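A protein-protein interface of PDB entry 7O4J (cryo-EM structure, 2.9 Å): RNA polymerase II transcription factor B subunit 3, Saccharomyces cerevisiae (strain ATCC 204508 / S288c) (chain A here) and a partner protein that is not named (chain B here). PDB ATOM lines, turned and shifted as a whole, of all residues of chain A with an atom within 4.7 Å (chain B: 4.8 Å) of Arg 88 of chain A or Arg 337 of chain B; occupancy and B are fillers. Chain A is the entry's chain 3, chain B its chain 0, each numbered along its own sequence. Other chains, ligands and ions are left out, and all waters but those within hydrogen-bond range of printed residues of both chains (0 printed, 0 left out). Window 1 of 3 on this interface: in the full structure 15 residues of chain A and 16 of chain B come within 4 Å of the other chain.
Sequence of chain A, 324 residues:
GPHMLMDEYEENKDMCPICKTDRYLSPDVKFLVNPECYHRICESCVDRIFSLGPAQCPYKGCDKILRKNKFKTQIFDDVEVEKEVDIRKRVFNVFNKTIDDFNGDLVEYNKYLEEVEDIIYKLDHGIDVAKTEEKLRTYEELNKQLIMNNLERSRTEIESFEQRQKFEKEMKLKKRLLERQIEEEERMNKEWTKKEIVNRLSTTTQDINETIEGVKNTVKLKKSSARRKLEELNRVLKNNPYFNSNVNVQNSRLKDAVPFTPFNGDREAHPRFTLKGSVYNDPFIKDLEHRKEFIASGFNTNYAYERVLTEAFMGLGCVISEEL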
ATOM      1  N   VAL A  81      14.527 -16.741 -26.459  1.00  0.00           N
ATOM      2  CA  VAL A  81      13.417 -16.590 -27.392  1.00  0.00           C
ATOM      3  C   VAL A  81      12.738 -17.930 -27.640  1.00  0.00           C
ATOM      4  O   VAL A  81      11.514 -17.990 -27.814  1.00  0.00           O
ATOM      5  CB  VAL A  81      13.907 -15.949 -28.703  1.00  0.00           C
ATOM      6  CG1 VAL A  81      12.765 -15.849 -29.706  1.00  0.00           C
ATOM      7  CG2 VAL A  81      14.503 -14.577 -28.423  1.00  0.00           C
ATOM      8  N   GLU A  84      10.251 -18.413 -24.873  1.00  0.00           N
ATOM      9  CA  GLU A  84       9.077 -17.561 -25.027  1.00  0.00           C
ATOM     10  C   GLU A  84       8.178 -18.054 -26.153  1.00  0.00           C
ATOM     11  O   GLU A  84       6.951 -18.092 -26.007  1.00  0.00           O
ATOM     12  CB  GLU A  84       9.512 -16.118 -25.283  1.00  0.00           C
ATOM     13  CG  GLU A  84       8.412 -15.092 -25.066  1.00  0.00           C
ATOM     14  CD  GLU A  84       8.954 -13.739 -24.647  1.00  0.00           C
ATOM     15  OE1 GLU A  84       9.960 -13.293 -25.236  1.00  0.00           O
ATOM     16  OE2 GLU A  84       8.375 -13.124 -23.726  1.00  0.00           O
ATOM     17  N   VAL A  85       8.770 -18.439 -27.285  1.00  0.00           N
ATOM     18  CA  VAL A  85       7.971 -18.887 -28.422  1.00  0.00           C
ATOM     19  C   VAL A  85       7.217 -20.164 -28.077  1.00  0.00           C
ATOM     20  O   VAL A  85       6.026 -20.298 -28.383  1.00  0.00           O
ATOM     21  CB  VAL A  85       8.867 -19.075 -29.659  1.00  0.00           C
ATOM     22  CG1 VAL A  85       8.108 -19.795 -30.762  1.00  0.00           C
ATOM     23  CG2 VAL A  85       9.375 -17.731 -30.152  1.00  0.00           C
ATOM     24  N   ASP A  86       7.891 -21.122 -27.439  1.00  0.00           N
ATOM     25  CA  ASP A  86       7.229 -22.373 -27.086  1.00  0.00           C
ATOM     26  C   ASP A  86       6.080 -22.132 -26.115  1.00  0.00           C
ATOM     27  O   ASP A  86       4.999 -22.714 -26.264  1.00  0.00           O
ATOM     28  CB  ASP A  86       8.241 -23.351 -26.493  1.00  0.00           C
ATOM     29  CG  ASP A  86       9.215 -23.874 -27.528  1.00  0.00           C
ATOM     30  OD1 ASP A  86       9.490 -23.149 -28.508  1.00  0.00           O
ATOM     31  OD2 ASP A  86       9.708 -25.009 -27.362  1.00  0.00           O
ATOM     32  N   ILE A  87       6.292 -21.277 -25.113  1.00  0.00           N
ATOM     33  CA  ILE A  87       5.200 -20.911 -24.217  1.00  0.00           C
ATOM     34  C   ILE A  87       4.107 -20.188 -24.991  1.00  0.00           C
ATOM     35  O   ILE A  87       2.912 -20.398 -24.754  1.00  0.00           O
ATOM     36  CB  ILE A  87       5.726 -20.058 -23.048  1.00  0.00           C
ATOM     37  CG1 ILE A  87       6.700 -20.877 -22.195  1.00  0.00           C
ATOM     38  CG2 ILE A  87       4.567 -19.545 -22.201  1.00  0.00           C
ATOM     39  CD1 ILE A  87       7.411 -20.075 -21.125  1.00  0.00           C
ATOM     40  N   ARG A  88       4.499 -19.327 -25.932  1.00  0.00           N
ATOM     41  CA  ARG A  88       3.515 -18.650 -26.770  1.00  0.00           C
ATOM     42  C   ARG A  88       2.696 -19.654 -27.569  1.00  0.00           C
ATOM     43  O   ARG A  88       1.475 -19.511 -27.697  1.00  0.00           O
ATOM     44  CB  ARG A  88       4.220 -17.666 -27.704  1.00  0.00           C
ATOM     45  CG  ARG A  88       3.279 -16.771 -28.495  1.00  0.00           C
ATOM     46  CD  ARG A  88       4.010 -15.578 -29.094  1.00  0.00           C
ATOM     47  NE  ARG A  88       4.689 -14.774 -28.082  1.00  0.00           N
ATOM     48  CZ  ARG A  88       4.132 -13.764 -27.419  1.00  0.00           C
ATOM     49  NH1 ARG A  88       2.873 -13.418 -27.649  1.00  0.00           N
ATOM     50  NH2 ARG A  88       4.840 -13.098 -26.519  1.00  0.00           N
ATOM     51  N   LYS A  89       3.354 -20.678 -28.118  1.00  0.00           N
ATOM     52  CA  LYS A  89       2.631 -21.719 -28.839  1.00  0.00           C
ATOM     53  C   LYS A  89       1.679 -22.466 -27.914  1.00  0.00           C
ATOM     54  O   LYS A  89       0.548 -22.782 -28.301  1.00  0.00           O
ATOM     55  CB  LYS A  89       3.623 -22.684 -29.487  1.00  0.00           C
ATOM     56  CG  LYS A  89       2.973 -23.774 -30.328  1.00  0.00           C
ATOM     57  CD  LYS A  89       3.854 -24.232 -31.495  1.00  0.00           C
ATOM     58  CE  LYS A  89       5.328 -24.370 -31.114  1.00  0.00           C
ATOM     59  NZ  LYS A  89       6.149 -24.862 -32.256  1.00  0.00           N
ATOM     60  N   ARG A  90       2.120 -22.760 -26.690  1.00  0.00           N
ATOM     61  CA  ARG A  90       1.256 -23.453 -25.740  1.00  0.00           C
ATOM     62  C   ARG A  90       0.025 -22.619 -25.402  1.00  0.00           C
ATOM     63  O   ARG A  90      -1.094 -23.142 -25.365  1.00  0.00           O
ATOM     64  CB  ARG A  90       2.040 -23.786 -24.471  1.00  0.00           C
ATOM     65  CG  ARG A  90       1.298 -24.686 -23.493  1.00  0.00           C
ATOM     66  CD  ARG A  90       1.789 -24.483 -22.068  1.00  0.00           C
ATOM     67  NE  ARG A  90       3.241 -24.347 -21.996  1.00  0.00           N
ATOM     68  CZ  ARG A  90       3.918 -24.121 -20.874  1.00  0.00           C
ATOM     69  NH1 ARG A  90       3.276 -24.005 -19.718  1.00  0.00           N
ATOM     70  NH2 ARG A  90       5.238 -24.012 -20.906  1.00  0.00           N
ATOM     71  N   VAL A  91       0.211 -21.323 -25.154  1.00  0.00           N
ATOM     72  CA  VAL A  91      -0.914 -20.471 -24.786  1.00  0.00           C
ATOM     73  C   VAL A  91      -1.844 -20.260 -25.974  1.00  0.00           C
ATOM     74  O   VAL A  91      -3.069 -20.334 -25.835  1.00  0.00           O
ATOM     75  CB  VAL A  91      -0.403 -19.131 -24.224  1.00  0.00           C
ATOM     76  CG1 VAL A  91      -1.568 -18.196 -23.941  1.00  0.00           C
ATOM     77  CG2 VAL A  91       0.412 -19.362 -22.962  1.00  0.00           C
ATOM     78  N   PHE A  92      -1.287 -19.998 -27.158  1.00  0.00           N
ATOM     79  CA  PHE A  92      -2.115 -19.783 -28.337  1.00  0.00           C
ATOM     80  C   PHE A  92      -2.873 -21.034 -28.756  1.00  0.00           C
ATOM     81  O   PHE A  92      -3.851 -20.921 -29.502  1.00  0.00           O
ATOM     82  CB  PHE A  92      -1.257 -19.284 -29.504  1.00  0.00           C
ATOM     83  CG  PHE A  92      -0.796 -17.853 -29.365  1.00  0.00           C
ATOM     84  CD1 PHE A  92      -1.251 -17.043 -28.333  1.00  0.00           C
ATOM     85  CD2 PHE A  92       0.093 -17.315 -30.280  1.00  0.00           C
ATOM     86  CE1 PHE A  92      -0.824 -15.736 -28.219  1.00  0.00           C
ATOM     87  CE2 PHE A  92       0.520 -16.006 -30.167  1.00  0.00           C
ATOM     88  CZ  PHE A  92       0.061 -15.217 -29.136  1.00  0.00           C
ATOM     89  N   GLU A 117      -0.757 -11.556 -23.674  1.00  0.00           N
ATOM     90  CA  GLU A 117       0.657 -11.213 -23.551  1.00  0.00           C
ATOM     91  C   GLU A 117       1.094 -11.213 -22.092  1.00  0.00           C
ATOM     92  O   GLU A 117       2.186 -11.689 -21.765  1.00  0.00           O
ATOM     93  CB  GLU A 117       0.926  -9.852 -24.190  1.00  0.00           C
ATOM     94  CG  GLU A 117       0.575  -9.777 -25.667  1.00  0.00           C
ATOM     95  CD  GLU A 117       1.694 -10.277 -26.562  1.00  0.00           C
ATOM     96  OE1 GLU A 117       2.864  -9.923 -26.309  1.00  0.00           O
ATOM     97  OE2 GLU A 117       1.400 -11.025 -27.519  1.00  0.00           O
ATOM     98  N   ILE A 120       1.578 -14.758 -21.078  1.00  0.00           N
ATOM     99  CA  ILE A 120       2.828 -15.289 -21.615  1.00  0.00           C
ATOM    100  C   ILE A 120       4.014 -14.738 -20.838  1.00  0.00           C
ATOM    101  O   ILE A 120       4.955 -15.471 -20.509  1.00  0.00           O
ATOM    102  CB  ILE A 120       2.937 -14.973 -23.118  1.00  0.00           C
ATOM    103  CG1 ILE A 120       1.895 -15.781 -23.896  1.00  0.00           C
ATOM    104  CG2 ILE A 120       4.348 -15.268 -23.621  1.00  0.00           C
ATOM    105  CD1 ILE A 120       1.816 -15.440 -25.367  1.00  0.00           C
ATOM    106  N   SER B 333       9.964  -7.981 -26.421  1.00  0.00           N
ATOM    107  CA  SER B 333       9.932  -9.396 -26.770  1.00  0.00           C
ATOM    108  C   SER B 333       9.454  -9.590 -28.202  1.00  0.00           C
ATOM    109  O   SER B 333      10.009 -10.407 -28.947  1.00  0.00           O
ATOM    110  CB  SER B 333       9.032 -10.158 -25.798  1.00  0.00           C
ATOM    111  OG  SER B 333       7.680  -9.760 -25.942  1.00  0.00           O
ATOM    112  N   PHE B 334       8.422  -8.846 -28.604  1.00  0.00           N
ATOM    113  CA  PHE B 334       7.979  -8.867 -29.994  1.00  0.00           C
ATOM    114  C   PHE B 334       9.127  -8.508 -30.928  1.00  0.00           C
ATOM    115  O   PHE B 334       9.334  -9.154 -31.961  1.00  0.00           O
ATOM    116  CB  PHE B 334       6.807  -7.898 -30.170  1.00  0.00           C
ATOM    117  CG  PHE B 334       6.347  -7.738 -31.592  1.00  0.00           C
ATOM    118  CD1 PHE B 334       6.995  -6.869 -32.453  1.00  0.00           C
ATOM    119  CD2 PHE B 334       5.255  -8.446 -32.063  1.00  0.00           C
ATOM    120  CE1 PHE B 334       6.572  -6.717 -33.756  1.00  0.00           C
ATOM    121  CE2 PHE B 334       4.827  -8.296 -33.366  1.00  0.00           C
ATOM    122  CZ  PHE B 334       5.487  -7.431 -34.213  1.00  0.00           C
ATOM    123  N   LEU B 335       9.884  -7.470 -30.574  1.00  0.00           N
ATOM    124  CA  LEU B 335      10.995  -7.038 -31.413  1.00  0.00           C
ATOM    125  C   LEU B 335      12.115  -8.073 -31.429  1.00  0.00           C
ATOM    126  O   LEU B 335      12.712  -8.337 -32.479  1.00  0.00           O
ATOM    127  CB  LEU B 335      11.511  -5.688 -30.919  1.00  0.00           C
ATOM    128  CG  LEU B 335      12.637  -5.016 -31.702  1.00  0.00           C
ATOM    129  CD1 LEU B 335      12.241  -4.789 -33.152  1.00  0.00           C
ATOM    130  CD2 LEU B 335      13.002  -3.703 -31.029  1.00  0.00           C
ATOM    131  N   LYS B 336      12.418  -8.671 -30.274  1.00  0.00           N
ATOM    132  CA  LYS B 336      13.530  -9.614 -30.202  1.00  0.00           C
ATOM    133  C   LYS B 336      13.270 -10.856 -31.045  1.00  0.00           C
ATOM    134  O   LYS B 336      14.155 -11.312 -31.776  1.00  0.00           O
ATOM    135  CB  LYS B 336      13.801 -10.006 -28.750  1.00  0.00           C
ATOM    136  CG  LYS B 336      14.846  -9.140 -28.064  1.00  0.00           C
ATOM    137  CD  LYS B 336      15.312  -9.752 -26.751  1.00  0.00           C
ATOM    138  CE  LYS B 336      14.436  -9.321 -25.589  1.00  0.00           C
ATOM    139  NZ  LYS B 336      15.071  -9.613 -24.275  1.00  0.00           N
ATOM    140  N   ARG B 337      12.065 -11.425 -30.954  1.00  0.00           N
ATOM    141  CA  ARG B 337      11.789 -12.648 -31.698  1.00  0.00           C
ATOM    142  C   ARG B 337      11.616 -12.378 -33.186  1.00  0.00           C
ATOM    143  O   ARG B 337      11.813 -13.286 -34.002  1.00  0.00           O
ATOM    144  CB  ARG B 337      10.555 -13.351 -31.127  1.00  0.00           C
ATOM    145  CG  ARG B 337       9.242 -12.617 -31.305  1.00  0.00           C
ATOM    146  CD  ARG B 337       8.083 -13.487 -30.844  1.00  0.00           C
ATOM    147  NE  ARG B 337       6.796 -12.801 -30.927  1.00  0.00           N
ATOM    148  CZ  ARG B 337       6.260 -12.077 -29.950  1.00  0.00           C
ATOM    149  NH1 ARG B 337       6.896 -11.922 -28.796  1.00  0.00           N
ATOM    150  NH2 ARG B 337       5.082 -11.496 -30.130  1.00  0.00           N
ATOM    151  N   LEU B 338      11.244 -11.151 -33.561  1.00  0.00           N
ATOM    152  CA  LEU B 338      11.283 -10.773 -34.970  1.00  0.00           C
ATOM    153  C   LEU B 338      12.716 -10.768 -35.485  1.00  0.00           C
ATOM    154  O   LEU B 338      12.983 -11.207 -36.610  1.00  0.00           O
ATOM    155  CB  LEU B 338      10.634  -9.402 -35.164  1.00  0.00           C
ATOM    156  CG  LEU B 338      10.788  -8.743 -36.539  1.00  0.00           C
ATOM    157  CD1 LEU B 338       9.923  -9.440 -37.575  1.00  0.00           C
ATOM    158  CD2 LEU B 338      10.439  -7.266 -36.460  1.00  0.00           C
ATOM    159  N   ILE B 339      13.653 -10.269 -34.675  1.00  0.00           N
ATOM    160  CA  ILE B 339      15.058 -10.271 -35.071  1.00  0.00           C
ATOM    161  C   ILE B 339      15.566 -11.698 -35.212  1.00  0.00           C
ATOM    162  O   ILE B 339      16.320 -12.018 -36.138  1.00  0.00           O
ATOM    163  CB  ILE B 339      15.897  -9.468 -34.060  1.00  0.00           C
ATOM    164  CG1 ILE B 339      15.497  -7.992 -34.091  1.00  0.00           C
ATOM    165  CG2 ILE B 339      17.381  -9.624 -34.361  1.00  0.00           C
ATOM    166  CD1 ILE B 339      16.012  -7.192 -32.913  1.00  0.00           C
ATOM    167  N   GLU B 340      15.170 -12.578 -34.290  1.00  0.00           N
ATOM    168  CA  GLU B 340      15.601 -13.969 -34.368  1.00  0.00           C
ATOM    169  C   GLU B 340      15.110 -14.627 -35.650  1.00  0.00           C
ATOM    170  O   GLU B 340      15.852 -15.381 -36.290  1.00  0.00           O
ATOM    171  CB  GLU B 340      15.103 -14.742 -33.146  1.00  0.00           C
ATOM    172  CG  GLU B 340      15.768 -14.339 -31.843  1.00  0.00           C
ATOM    173  CD  GLU B 340      17.268 -14.554 -31.861  1.00  0.00           C
ATOM    174  OE1 GLU B 340      17.720 -15.524 -32.504  1.00  0.00           O
ATOM    175  OE2 GLU B 340      17.992 -13.753 -31.234  1.00  0.00           O
ATOM    176  N   TYR B 341      13.862 -14.359 -36.040  1.00  0.00           N
ATOM    177  CA  TYR B 341      13.347 -14.922 -37.283  1.00  0.00           C
ATOM    178  C   TYR B 341      14.131 -14.412 -38.484  1.00  0.00           C
ATOM    179  O   TYR B 341      14.389 -15.163 -39.431  1.00  0.00           O
ATOM    180  CB  TYR B 341      11.865 -14.595 -37.439  1.00  0.00           C
ATOM    181  CG  TYR B 341      11.302 -15.042 -38.766  1.00  0.00           C
ATOM    182  CD1 TYR B 341      11.006 -16.376 -39.004  1.00  0.00           C
ATOM    183  CD2 TYR B 341      11.077 -14.130 -39.786  1.00  0.00           C
ATOM    184  CE1 TYR B 341      10.497 -16.787 -40.218  1.00  0.00           C
ATOM    185  CE2 TYR B 341      10.568 -14.531 -41.000  1.00  0.00           C
ATOM    186  CZ  TYR B 341      10.281 -15.858 -41.212  1.00  0.00           C
ATOM    187  OH  TYR B 341       9.774 -16.254 -42.426  1.00  0.00           O
ATOM    188  N   THR B 367       7.094 -18.172 -35.771  1.00  0.00           N
ATOM    189  CA  THR B 367       6.655 -17.392 -34.626  1.00  0.00           C
ATOM    190  C   THR B 367       5.173 -17.071 -34.810  1.00  0.00           C
ATOM    191  O   THR B 367       4.513 -17.589 -35.714  1.00  0.00           O
ATOM    192  CB  THR B 367       7.507 -16.131 -34.463  1.00  0.00           C
ATOM    193  OG1 THR B 367       7.017 -15.365 -33.355  1.00  0.00           O
ATOM    194  CG2 THR B 367       7.471 -15.269 -35.715  1.00  0.00           C
ATOM    195  N   PHE B 368       4.636 -16.214 -33.948  1.00  0.00           N
ATOM    196  CA  PHE B 368       3.219 -15.865 -33.969  1.00  0.00           C
ATOM    197  C   PHE B 368       3.045 -14.356 -34.060  1.00  0.00           C
ATOM    198  O   PHE B 368       2.277 -13.740 -33.317  1.00  0.00           O
ATOM    199  CB  PHE B 368       2.516 -16.435 -32.742  1.00  0.00           C
ATOM    200  CG  PHE B 368       2.765 -17.899 -32.534  1.00  0.00           C
ATOM    201  CD1 PHE B 368       1.947 -18.844 -33.129  1.00  0.00           C
ATOM    202  CD2 PHE B 368       3.824 -18.333 -31.756  1.00  0.00           C
ATOM    203  CE1 PHE B 368       2.175 -20.192 -32.945  1.00  0.00           C
ATOM    204  CE2 PHE B 368       4.057 -19.681 -31.569  1.00  0.00           C
ATOM    205  CZ  PHE B 368       3.232 -20.611 -32.163  1.00  0.00           C
ATOM    206  N   ILE B 369       3.769 -13.741 -34.989  1.00  0.00           N
ATOM    207  CA  ILE B 369       3.665 -12.313 -35.263  1.00  0.00           C
ATOM    208  C   ILE B 369       2.701 -12.125 -36.426  1.00  0.00           C
ATOM    209  O   ILE B 369       2.887 -12.711 -37.499  1.00  0.00           O
ATOM    210  CB  ILE B 369       5.038 -11.701 -35.582  1.00  0.00           C
ATOM    211  CG1 ILE B 369       5.924 -11.715 -34.334  1.00  0.00           C
ATOM    212  CG2 ILE B 369       4.870 -10.285 -36.122  1.00  0.00           C
ATOM    213  CD1 ILE B 369       7.381 -11.413 -34.608  1.00  0.00           C
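Among the printed residues, merely in contact across the chains: Phe 92 of chain A with Phe 368 of chain B (3.3 Å), Glu 84 of chain A with Ser 333 of chain B (3.3 Å), Lys 89 of chain A with Phe 368 of chain B (3.4 Å), Val 81 of chain A with Arg 337 of chain B (3.6 Å), Val 81 of chain A with Glu 340 of chain B (3.7 Å), Arg 88 of chain A with Phe 368 of chain B (3.7 Å) and Val 85 of chain A with Phe 368 of chain B (3.8 Å).
NH2 of Arg 88 of chain A sits close to NH1 of Arg 337 of chain B.
Hydrophobic or aromatic side chains of chain A that line the printed part of chain B: Val 81 and Phe 92.
Arg 88 of chain A touches just these residues of chain B: Arg 337 (3.3 Å) and Phe 368 (3.7 Å).
Arg 337 of chain B touches just these residues of chain A: Val 81 and Arg 88.
Of the printed residues of chain B, Lys 89 of chain A touches Phe 368.
Printed residues of chain B within 4 Å of Val 81 of chain A: Arg 337 and Glu 340.
Of the printed residues of chain B, Val 85 of chain A touches Phe 368 (3.8 Å).
The nearest residue of chain A that does not touch Arg 337 of chain B is Val 85 of chain A (4.5 Å).
The guanidinium group (NH1) of Arg 88 of chain A lies within salt-bridge range of the side-chain carboxylate (OE2) of Glu 117 of chain A (2.8 Å).
The backbone carbonyl oxygen (O) of Ser 333 of chain B lies close to the guanidinium group (NH1) of Arg 337 of chain B, 3.5 Å away.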
